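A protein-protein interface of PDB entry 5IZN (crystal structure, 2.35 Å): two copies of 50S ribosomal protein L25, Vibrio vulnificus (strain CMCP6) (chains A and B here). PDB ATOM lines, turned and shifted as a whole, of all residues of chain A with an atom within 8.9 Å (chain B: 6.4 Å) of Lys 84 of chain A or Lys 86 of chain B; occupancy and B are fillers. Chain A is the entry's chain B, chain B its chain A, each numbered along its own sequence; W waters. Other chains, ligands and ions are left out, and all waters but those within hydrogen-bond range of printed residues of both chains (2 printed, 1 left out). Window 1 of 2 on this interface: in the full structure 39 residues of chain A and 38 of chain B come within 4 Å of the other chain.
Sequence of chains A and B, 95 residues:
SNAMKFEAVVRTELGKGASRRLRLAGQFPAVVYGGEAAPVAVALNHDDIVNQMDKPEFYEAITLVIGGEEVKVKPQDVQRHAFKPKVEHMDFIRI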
ATOM      1  N   ARG A  23      26.973  -7.263  11.696  1.00  0.00           N
ATOM      2  CA  ARG A  23      25.623  -7.560  11.228  1.00  0.00           C
ATOM      3  C   ARG A  23      24.778  -8.210  12.319  1.00  0.00           C
ATOM      4  O   ARG A  23      23.603  -7.880  12.483  1.00  0.00           O
ATOM      5  CB  ARG A  23      25.664  -8.465   9.996  1.00  0.00           C
ATOM      6  CG  ARG A  23      24.291  -8.759   9.413  1.00  0.00           C
ATOM      7  CD  ARG A  23      24.384  -9.584   8.143  1.00  0.00           C
ATOM      8  NE  ARG A  23      24.952 -10.905   8.387  1.00  0.00           N
ATOM      9  CZ  ARG A  23      24.239 -11.974   8.728  1.00  0.00           C
ATOM     10  NH1 ARG A  23      22.923 -11.879   8.868  1.00  0.00           N
ATOM     11  NH2 ARG A  23      24.841 -13.138   8.929  1.00  0.00           N
ATOM     12  N   LEU A  24      25.381  -9.129  13.069  1.00  0.00           N
ATOM     13  CA  LEU A  24      24.676  -9.794  14.159  1.00  0.00           C
ATOM     14  C   LEU A  24      24.544  -8.869  15.365  1.00  0.00           C
ATOM     15  O   LEU A  24      23.824  -9.171  16.315  1.00  0.00           O
ATOM     16  CB  LEU A  24      25.387 -11.089  14.556  1.00  0.00           C
ATOM     17  CG  LEU A  24      25.466 -12.169  13.473  1.00  0.00           C
ATOM     18  CD1 LEU A  24      25.923 -13.494  14.064  1.00  0.00           C
ATOM     19  CD2 LEU A  24      24.130 -12.325  12.767  1.00  0.00           C
ATOM     20  N   PHE A  28      26.713  -2.277  10.410  1.00  0.00           N
ATOM     21  CA  PHE A  28      27.389  -2.562   9.149  1.00  0.00           C
ATOM     22  C   PHE A  28      28.564  -1.603   8.961  1.00  0.00           C
ATOM     23  O   PHE A  28      28.514  -0.460   9.416  1.00  0.00           O
ATOM     24  CB  PHE A  28      26.412  -2.468   7.970  1.00  0.00           C
ATOM     25  CG  PHE A  28      26.062  -1.060   7.574  1.00  0.00           C
ATOM     26  CD1 PHE A  28      25.071  -0.364   8.244  1.00  0.00           C
ATOM     27  CD2 PHE A  28      26.712  -0.441   6.518  1.00  0.00           C
ATOM     28  CE1 PHE A  28      24.743   0.928   7.877  1.00  0.00           C
ATOM     29  CE2 PHE A  28      26.389   0.851   6.148  1.00  0.00           C
ATOM     30  CZ  PHE A  28      25.403   1.536   6.827  1.00  0.00           C
ATOM     31  N   HIS A  46      22.472  -0.335  11.342  1.00  0.00           N
ATOM     32  CA  HIS A  46      21.954  -0.757  10.046  1.00  0.00           C
ATOM     33  C   HIS A  46      20.542  -0.247   9.773  1.00  0.00           C
ATOM     34  O   HIS A  46      20.332   0.562   8.870  1.00  0.00           O
ATOM     35  CB  HIS A  46      21.974  -2.283   9.940  1.00  0.00           C
ATOM     36  CG  HIS A  46      21.471  -2.801   8.630  1.00  0.00           C
ATOM     37  ND1 HIS A  46      20.143  -3.095   8.406  1.00  0.00           N
ATOM     38  CD2 HIS A  46      22.116  -3.070   7.470  1.00  0.00           C
ATOM     39  CE1 HIS A  46      19.993  -3.528   7.167  1.00  0.00           C
ATOM     40  NE2 HIS A  46      21.175  -3.523   6.579  1.00  0.00           N
ATOM     41  N   ASP A  47      19.580  -0.721  10.560  1.00  0.00           N
ATOM     42  CA  ASP A  47      18.174  -0.401  10.332  1.00  0.00           C
ATOM     43  C   ASP A  47      17.878   1.090  10.472  1.00  0.00           C
ATOM     44  O   ASP A  47      16.953   1.603   9.845  1.00  0.00           O
ATOM     45  CB  ASP A  47      17.290  -1.198  11.292  1.00  0.00           C
ATOM     46  CG  ASP A  47      17.387  -2.690  11.068  1.00  0.00           C
ATOM     47  OD1 ASP A  47      17.807  -3.098   9.964  1.00  0.00           O
ATOM     48  OD2 ASP A  47      17.040  -3.454  11.993  1.00  0.00           O
ATOM     49  N   VAL A  50      19.267   2.530   7.075  1.00  0.00           N
ATOM     50  CA  VAL A  50      18.445   2.019   5.982  1.00  0.00           C
ATOM     51  C   VAL A  50      17.070   2.687   5.922  1.00  0.00           C
ATOM     52  O   VAL A  50      16.555   2.972   4.839  1.00  0.00           O
ATOM     53  CB  VAL A  50      18.269   0.486   6.102  1.00  0.00           C
ATOM     54  CG1 VAL A  50      17.183  -0.019   5.166  1.00  0.00           C
ATOM     55  CG2 VAL A  50      19.587  -0.218   5.822  1.00  0.00           C
ATOM     56  N   MET A  53      16.989   5.814   3.818  1.00  0.00           N
ATOM     57  CA  MET A  53      17.523   5.750   2.462  1.00  0.00           C
ATOM     58  C   MET A  53      16.443   5.863   1.389  1.00  0.00           C
ATOM     59  O   MET A  53      16.722   5.707   0.200  1.00  0.00           O
ATOM     60  CB  MET A  53      18.316   4.458   2.271  1.00  0.00           C
ATOM     61  CG  MET A  53      19.529   4.358   3.177  1.00  0.00           C
ATOM     62  SD  MET A  53      20.638   2.809   2.788  1.00  0.00           S
ATOM     63  CE  MET A  53      21.130   3.248   0.953  1.00  0.00           C
ATOM     64  N   VAL A  78      28.876   4.343  -5.378  1.00  0.00           N
ATOM     65  CA  VAL A  78      30.045   3.580  -5.805  1.00  0.00           C
ATOM     66  C   VAL A  78      29.690   2.140  -6.156  1.00  0.00           C
ATOM     67  O   VAL A  78      29.886   1.702  -7.290  1.00  0.00           O
ATOM     68  CB  VAL A  78      31.136   3.572  -4.721  1.00  0.00           C
ATOM     69  CG1 VAL A  78      32.322   2.736  -5.171  1.00  0.00           C
ATOM     70  CG2 VAL A  78      31.570   4.993  -4.397  1.00  0.00           C
ATOM     71  N   GLN A  79      29.176   1.403  -5.176  1.00  0.00           N
ATOM     72  CA  GLN A  79      28.775   0.018  -5.388  1.00  0.00           C
ATOM     73  C   GLN A  79      27.592  -0.056  -6.346  1.00  0.00           C
ATOM     74  O   GLN A  79      26.710   0.801  -6.322  1.00  0.00           O
ATOM     75  CB  GLN A  79      28.429  -0.650  -4.057  1.00  0.00           C
ATOM     76  CG  GLN A  79      27.418   0.119  -3.223  1.00  0.00           C
ATOM     77  CD  GLN A  79      27.233  -0.467  -1.836  1.00  0.00           C
ATOM     78  OE1 GLN A  79      27.676  -1.580  -1.553  1.00  0.00           O
ATOM     79  NE2 GLN A  79      26.579   0.286  -0.960  1.00  0.00           N
ATOM     80  N   ARG A  80      27.583  -1.082  -7.191  1.00  0.00           N
ATOM     81  CA  ARG A  80      26.526  -1.249  -8.182  1.00  0.00           C
ATOM     82  C   ARG A  80      25.173  -1.468  -7.513  1.00  0.00           C
ATOM     83  O   ARG A  80      24.190  -0.806  -7.850  1.00  0.00           O
ATOM     84  CB  ARG A  80      26.847  -2.417  -9.117  1.00  0.00           C
ATOM     85  CG  ARG A  80      25.795  -2.661 -10.186  1.00  0.00           C
ATOM     86  CD  ARG A  80      25.565  -1.417 -11.030  1.00  0.00           C
ATOM     87  NE  ARG A  80      24.463  -1.593 -11.972  1.00  0.00           N
ATOM     88  CZ  ARG A  80      23.185  -1.384 -11.672  1.00  0.00           C
ATOM     89  NH1 ARG A  80      22.843  -0.992 -10.452  1.00  0.00           N
ATOM     90  NH2 ARG A  80      22.247  -1.568 -12.592  1.00  0.00           N
ATOM     91  N   HIS A  81      25.130  -2.395  -6.563  1.00  0.00           N
ATOM     92  CA  HIS A  81      23.904  -2.674  -5.825  1.00  0.00           C
ATOM     93  C   HIS A  81      24.105  -2.443  -4.332  1.00  0.00           C
ATOM     94  O   HIS A  81      24.709  -3.266  -3.644  1.00  0.00           O
ATOM     95  CB  HIS A  81      23.435  -4.109  -6.078  1.00  0.00           C
ATOM     96  CG  HIS A  81      23.092  -4.389  -7.508  1.00  0.00           C
ATOM     97  ND1 HIS A  81      23.913  -5.118  -8.342  1.00  0.00           N
ATOM     98  CD2 HIS A  81      22.020  -4.032  -8.253  1.00  0.00           C
ATOM     99  CE1 HIS A  81      23.358  -5.201  -9.539  1.00  0.00           C
ATOM    100  NE2 HIS A  81      22.210  -4.550  -9.512  1.00  0.00           N
ATOM    101  N   ALA A  82      23.596  -1.319  -3.838  1.00  0.00           N
ATOM    102  CA  ALA A  82      23.713  -0.981  -2.424  1.00  0.00           C
ATOM    103  C   ALA A  82      22.928  -1.966  -1.566  1.00  0.00           C
ATOM    104  O   ALA A  82      23.314  -2.264  -0.434  1.00  0.00           O
ATOM    105  CB  ALA A  82      23.232   0.440  -2.177  1.00  0.00           C
ATOM    106  N   PHE A  83      21.826  -2.466  -2.112  1.00  0.00           N
ATOM    107  CA  PHE A  83      20.982  -3.414  -1.399  1.00  0.00           C
ATOM    108  C   PHE A  83      21.252  -4.839  -1.865  1.00  0.00           C
ATOM    109  O   PHE A  83      21.357  -5.107  -3.061  1.00  0.00           O
ATOM    110  CB  PHE A  83      19.509  -3.053  -1.579  1.00  0.00           C
ATOM    111  CG  PHE A  83      19.136  -1.739  -0.959  1.00  0.00           C
ATOM    112  CD1 PHE A  83      18.757  -1.671   0.372  1.00  0.00           C
ATOM    113  CD2 PHE A  83      19.181  -0.571  -1.699  1.00  0.00           C
ATOM    114  CE1 PHE A  83      18.419  -0.462   0.949  1.00  0.00           C
ATOM    115  CE2 PHE A  83      18.846   0.641  -1.126  1.00  0.00           C
ATOM    116  CZ  PHE A  83      18.464   0.695   0.199  1.00  0.00           C
ATOM    117  N   LYS A  84      21.362  -5.748  -0.904  1.00  0.00           N
ATOM    118  CA  LYS A  84      21.786  -7.115  -1.170  1.00  0.00           C
ATOM    119  C   LYS A  84      20.590  -8.068  -1.226  1.00  0.00           C
ATOM    120  O   LYS A  84      19.521  -7.741  -0.712  1.00  0.00           O
ATOM    121  CB  LYS A  84      22.793  -7.552  -0.101  1.00  0.00           C
ATOM    122  CG  LYS A  84      24.012  -6.643  -0.025  1.00  0.00           C
ATOM    123  CD  LYS A  84      24.574  -6.360  -1.415  1.00  0.00           C
ATOM    124  CE  LYS A  84      25.731  -5.378  -1.364  1.00  0.00           C
ATOM    125  NZ  LYS A  84      26.301  -5.110  -2.716  1.00  0.00           N
ATOM    126  N   PRO A  85      20.763  -9.237  -1.876  1.00  0.00           N
ATOM    127  CA  PRO A  85      19.704 -10.240  -2.038  1.00  0.00           C
ATOM    128  C   PRO A  85      18.886 -10.527  -0.779  1.00  0.00           C
ATOM    129  O   PRO A  85      19.423 -10.608   0.327  1.00  0.00           O
ATOM    130  CB  PRO A  85      20.483 -11.484  -2.464  1.00  0.00           C
ATOM    131  CG  PRO A  85      21.598 -10.936  -3.266  1.00  0.00           C
ATOM    132  CD  PRO A  85      21.976  -9.620  -2.625  1.00  0.00           C
ATOM    133  N   LYS A  86      17.580 -10.674  -0.974  1.00  0.00           N
ATOM    134  CA  LYS A  86      16.643 -10.949   0.107  1.00  0.00           C
ATOM    135  C   LYS A  86      16.895 -12.320   0.732  1.00  0.00           C
ATOM    136  O   LYS A  86      16.991 -12.450   1.952  1.00  0.00           O
ATOM    137  CB  LYS A  86      15.207 -10.863  -0.419  1.00  0.00           C
ATOM    138  CG  LYS A  86      14.122 -10.942   0.641  1.00  0.00           C
ATOM    139  CD  LYS A  86      12.764 -11.169  -0.010  1.00  0.00           C
ATOM    140  CE  LYS A  86      11.627 -11.002   0.982  1.00  0.00           C
ATOM    141  NZ  LYS A  86      11.469  -9.582   1.397  1.00  0.00           N
ATOM    142  N   VAL A  87      17.010 -13.338  -0.114  1.00  0.00           N
ATOM    143  CA  VAL A  87      17.180 -14.711   0.353  1.00  0.00           C
ATOM    144  C   VAL A  87      18.599 -15.221   0.119  1.00  0.00           C
ATOM    145  O   VAL A  87      19.123 -15.144  -0.992  1.00  0.00           O
ATOM    146  CB  VAL A  87      16.183 -15.659  -0.341  1.00  0.00           C
ATOM    147  CG1 VAL A  87      16.432 -17.099   0.081  1.00  0.00           C
ATOM    148  CG2 VAL A  87      14.755 -15.244  -0.028  1.00  0.00           C
ATOM    149  N   GLU A  88      19.213 -15.742   1.177  1.00  0.00           N
ATOM    150  CA  GLU A  88      20.570 -16.270   1.099  1.00  0.00           C
ATOM    151  C   GLU A  88      20.559 -17.798   1.111  1.00  0.00           C
ATOM    152  O   GLU A  88      21.483 -18.443   0.614  1.00  0.00           O
ATOM    153  CB  GLU A  88      21.415 -15.726   2.254  1.00  0.00           C
ATOM    154  CG  GLU A  88      22.906 -15.994   2.127  1.00  0.00           C
ATOM    155  CD  GLU A  88      23.721 -15.238   3.158  1.00  0.00           C
ATOM    156  OE1 GLU A  88      23.175 -14.305   3.784  1.00  0.00           O
ATOM    157  OE2 GLU A  88      24.909 -15.578   3.345  1.00  0.00           O
ATOM    158  N   ARG B  23      25.477 -16.379  -5.952  1.00  0.00           N
ATOM    159  CA  ARG B  23      24.931 -15.053  -5.685  1.00  0.00           C
ATOM    160  C   ARG B  23      25.251 -14.075  -6.812  1.00  0.00           C
ATOM    161  O   ARG B  23      24.407 -13.269  -7.205  1.00  0.00           O
ATOM    162  CB  ARG B  23      25.464 -14.518  -4.355  1.00  0.00           C
ATOM    163  CG  ARG B  23      25.130 -13.061  -4.089  1.00  0.00           C
ATOM    164  CD  ARG B  23      25.748 -12.592  -2.784  1.00  0.00           C
ATOM    165  NE  ARG B  23      25.751 -11.137  -2.670  1.00  0.00           N
ATOM    166  CZ  ARG B  23      26.273 -10.471  -1.647  1.00  0.00           C
ATOM    167  NH1 ARG B  23      26.837 -11.129  -0.642  1.00  0.00           N
ATOM    168  NH2 ARG B  23      26.234  -9.146  -1.626  1.00  0.00           N
ATOM    169  N   HIS B  46      17.079 -16.468  -7.718  1.00  0.00           N
ATOM    170  CA  HIS B  46      16.699 -15.638  -6.580  1.00  0.00           C
ATOM    171  C   HIS B  46      15.402 -14.870  -6.818  1.00  0.00           C
ATOM    172  O   HIS B  46      14.432 -15.036  -6.079  1.00  0.00           O
ATOM    173  CB  HIS B  46      17.822 -14.655  -6.241  1.00  0.00           C
ATOM    174  CG  HIS B  46      17.521 -13.783  -5.063  1.00  0.00           C
ATOM    175  ND1 HIS B  46      16.905 -12.555  -5.185  1.00  0.00           N
ATOM    176  CD2 HIS B  46      17.746 -13.961  -3.741  1.00  0.00           C
ATOM    177  CE1 HIS B  46      16.768 -12.014  -3.988  1.00  0.00           C
ATOM    178  NE2 HIS B  46      17.269 -12.848  -3.094  1.00  0.00           N
ATOM    179  N   ALA B  82      12.187 -11.454  10.110  1.00  0.00           N
ATOM    180  CA  ALA B  82      11.539 -10.358   9.403  1.00  0.00           C
ATOM    181  C   ALA B  82      12.382  -9.945   8.204  1.00  0.00           C
ATOM    182  O   ALA B  82      13.601  -9.812   8.311  1.00  0.00           O
ATOM    183  CB  ALA B  82      11.311  -9.178  10.333  1.00  0.00           C
ATOM    184  N   LYS B  84      13.732  -7.359   5.542  1.00  0.00           N
ATOM    185  CA  LYS B  84      13.994  -5.934   5.449  1.00  0.00           C
ATOM    186  C   LYS B  84      15.101  -5.692   4.431  1.00  0.00           C
ATOM    187  O   LYS B  84      15.919  -6.578   4.187  1.00  0.00           O
ATOM    188  CB  LYS B  84      14.394  -5.380   6.817  1.00  0.00           C
ATOM    189  CG  LYS B  84      15.542  -6.145   7.454  1.00  0.00           C
ATOM    190  CD  LYS B  84      15.939  -5.571   8.801  1.00  0.00           C
ATOM    191  CE  LYS B  84      17.074  -6.376   9.414  1.00  0.00           C
ATOM    192  NZ  LYS B  84      17.511  -5.830  10.727  1.00  0.00           N
ATOM    193  N   PRO B  85      15.125  -4.497   3.822  1.00  0.00           N
ATOM    194  CA  PRO B  85      16.239  -4.157   2.929  1.00  0.00           C
ATOM    195  C   PRO B  85      17.568  -4.191   3.678  1.00  0.00           C
ATOM    196  O   PRO B  85      17.656  -3.673   4.792  1.00  0.00           O
ATOM    197  CB  PRO B  85      15.897  -2.738   2.454  1.00  0.00           C
ATOM    198  CG  PRO B  85      14.891  -2.225   3.438  1.00  0.00           C
ATOM    199  CD  PRO B  85      14.122  -3.422   3.890  1.00  0.00           C
ATOM    200  N   LYS B  86      18.583  -4.807   3.080  1.00  0.00           N
ATOM    201  CA  LYS B  86      19.859  -4.986   3.762  1.00  0.00           C
ATOM    202  C   LYS B  86      21.033  -4.359   3.019  1.00  0.00           C
ATOM    203  O   LYS B  86      21.126  -4.425   1.793  1.00  0.00           O
ATOM    204  CB  LYS B  86      20.130  -6.474   3.993  1.00  0.00           C
ATOM    205  CG  LYS B  86      19.229  -7.105   5.045  1.00  0.00           C
ATOM    206  CD  LYS B  86      19.715  -8.492   5.434  1.00  0.00           C
ATOM    207  CE  LYS B  86      18.891  -9.063   6.578  1.00  0.00           C
ATOM    208  NZ  LYS B  86      19.413 -10.381   7.036  1.00  0.00           N
ATOM    209  N   VAL B  87      21.928  -3.753   3.790  1.00  0.00           N
ATOM    210  CA  VAL B  87      23.131  -3.115   3.273  1.00  0.00           C
ATOM    211  C   VAL B  87      24.336  -3.633   4.054  1.00  0.00           C
ATOM    212  O   VAL B  87      24.268  -3.789   5.273  1.00  0.00           O
ATOM    213  CB  VAL B  87      23.038  -1.576   3.383  1.00  0.00           C
ATOM    214  CG1 VAL B  87      24.396  -0.926   3.164  1.00  0.00           C
ATOM    215  CG2 VAL B  87      22.009  -1.034   2.401  1.00  0.00           C
ATOM    216  N   GLU B  88      25.432  -3.919   3.357  1.00  0.00           N
ATOM    217  CA  GLU B  88      26.621  -4.446   4.017  1.00  0.00           C
ATOM    218  C   GLU B  88      27.815  -3.503   3.894  1.00  0.00           C
ATOM    219  O   GLU B  88      28.883  -3.772   4.443  1.00  0.00           O
ATOM    220  CB  GLU B  88      26.975  -5.824   3.452  1.00  0.00           C
ATOM    221  CG  GLU B  88      27.166  -5.858   1.948  1.00  0.00           C
ATOM    222  CD  GLU B  88      27.341  -7.270   1.420  1.00  0.00           C
ATOM    223  OE1 GLU B  88      27.726  -7.425   0.242  1.00  0.00           O
ATOM    224  OE2 GLU B  88      27.088  -8.226   2.182  1.00  0.00           O
ATOM    225  N   HIS B  89      27.624  -2.394   3.183  1.00  0.00           N
ATOM    226  CA  HIS B  89      28.680  -1.400   3.005  1.00  0.00           C
ATOM    227  C   HIS B  89      28.148  -0.092   2.423  1.00  0.00           C
ATOM    228  O   HIS B  89      27.218  -0.099   1.617  1.00  0.00           O
ATOM    229  CB  HIS B  89      29.784  -1.944   2.094  1.00  0.00           C
ATOM    230  CG  HIS B  89      30.783  -0.910   1.677  1.00  0.00           C
ATOM    231  ND1 HIS B  89      31.800  -0.483   2.502  1.00  0.00           N
ATOM    232  CD2 HIS B  89      30.909  -0.205   0.528  1.00  0.00           C
ATOM    233  CE1 HIS B  89      32.517   0.435   1.876  1.00  0.00           C
ATOM    234  NE2 HIS B  89      31.996   0.622   0.676  1.00  0.00           N
HETATM  235  O   HOH W   1      23.307  -6.213   6.874  1.00  0.00           O
HETATM  236  O   HOH W   2      16.642  -2.634   7.303  1.00  0.00           O
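A ring nitrogen (NE2) of His 46 of chain B sits at hydrogen-bond distance from the backbone NH (N) of Val 87 of chain A, 3.0 Å away. O of Lys 86 of chain B sits at hydrogen-bond distance from N of Lys 84 of chain A (3.0 Å). The side-chain amino group of Lys 84 of chain B is in salt-bridge range of the side-chain carboxylate of Asp 47 of chain A, 2.7 Å away. NE2 of Gln 79 of chain A sits at hydrogen-bond distance from O of His 89 of chain B (2.7 Å). A ring nitrogen (NE2) of His 46 of chain B is in hydrogen-bond range of the backbone NH (N) of Lys 86 of chain A (3.1 Å). A ring nitrogen (NE2) of His 46 of chain A lies within hydrogen-bond range of the backbone NH (N) of Val 87 of chain B, 2.9 Å away.
The guanidinium group (NH2) of Arg 23 of chain B is in salt-bridge range of the side-chain carboxylate (OE1) of Glu 88 of chain B, 2.9 Å away. A ring nitrogen (ND1) of His 46 of chain A is in hydrogen-bond range of the side-chain carboxylate (OD1) of Asp 47 of chain A (2.8 Å). The side-chain amino group (NZ) of Lys 84 of chain A lies within hydrogen-bond range of the backbone carbonyl oxygen (O) of His 81 of chain A (2.6 Å).
Among the printed residues, pairs that only touch across the chains: Phe 28 of chain A with Val 87 of chain B, Phe 28 of chain A with His 89 of chain B, His 46 of chain A with Pro 85 of chain B, His 46 of chain A with Lys 86 of chain B, Val 50 of chain A with Pro 85 of chain B, Ala 82 of chain A with Lys 86 of chain B, Ala 82 of chain A with Val 87 of chain B, Phe 83 of chain A with Pro 85 of chain B, Phe 83 of chain A with Lys 86 of chain B, Phe 83 of chain A with Val 87 of chain B, Lys 84 of chain A with Arg 23 of chain B, Lys 84 of chain A with Glu 88 of chain B and Pro 85 of chain A with His 46 of chain B.
Lys 84 of chain A touches just these residues of chain B: Arg 23 (3.2 Å), Lys 86 (3.0 Å) and Glu 88 (3.3 Å). Lys 86 of chain B touches four residues of chain A. Val 87 of chain B touches just these residues of chain A: Phe 28 (3.7 Å), His 46 (2.9 Å), Ala 82 (3.4 Å) and Phe 83 (3.9 Å). Of the printed residues of chain B, Val 50 of chain A touches Pro 85 (3.6 Å). Of the printed residues of chain A, Arg 23 of chain B touches Lys 84. Of the printed residues of chain B, Phe 28 of chain A touches Val 87 and His 89. Leu 24 of chain A touches none of the printed residues of chain B. The nearest printed residue of chain B that does not touch Gln 79 of chain A is Val 87 of chain B (4.8 Å).
Printed residues of chain A that touch a printed residue of chain B: Phe 28, His 46, Asp 47, Val 50, Gln 79, Ala 82, Phe 83, Lys 84, Pro 85, Lys 86 and Val 87. Hydrophobic or aromatic side chains of chain A that line the printed part of chain B: Phe 28, His 46, Val 50, Phe 83 and Pro 85. Along chain A the printed residues that touch a printed residue of chain B span positions 28 to 87. Printed residues of chain B that touch a printed residue of chain A: Arg 23, His 46, Lys 84, Pro 85, Lys 86, Val 87, Glu 88 and His 89. Among the printed residues, Asp or Glu carboxylates within 4 Å of a Lys or Arg side-chain nitrogen of the other chain: Asp 47 of chain A with Lys 84 of chain B.
His 46 of chain A touches Lys 86 of chain B, and with the chains exchanged Lys 86 of chain A touches His 46 of chain B. His 46 of chain A touches Val 87 of chain B, and with the chains exchanged Val 87 of chain A touches His 46 of chain B. Lys 84 of chain A touches Arg 23 of chain B, but with the chains exchanged Arg 23 of chain A does not touch Lys 84 of chain B (6.7 Å). Lys 84 of chain A touches Glu 88 of chain B, but with the chains exchanged Glu 88 of chain A does not touch Lys 84 of chain B (10.2 Å).
Water W2 lies within hydrogen-bond range of the backbone carbonyl oxygen (O) of Pro 85 of chain B and the side-chain carboxylate (OD1) of Asp 47 of chain A. Water W1 lies within hydrogen-bond range of O of Val 87 of chain B (3.1 Å) and NE2 of His 46 of chain A (3.4 Å).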
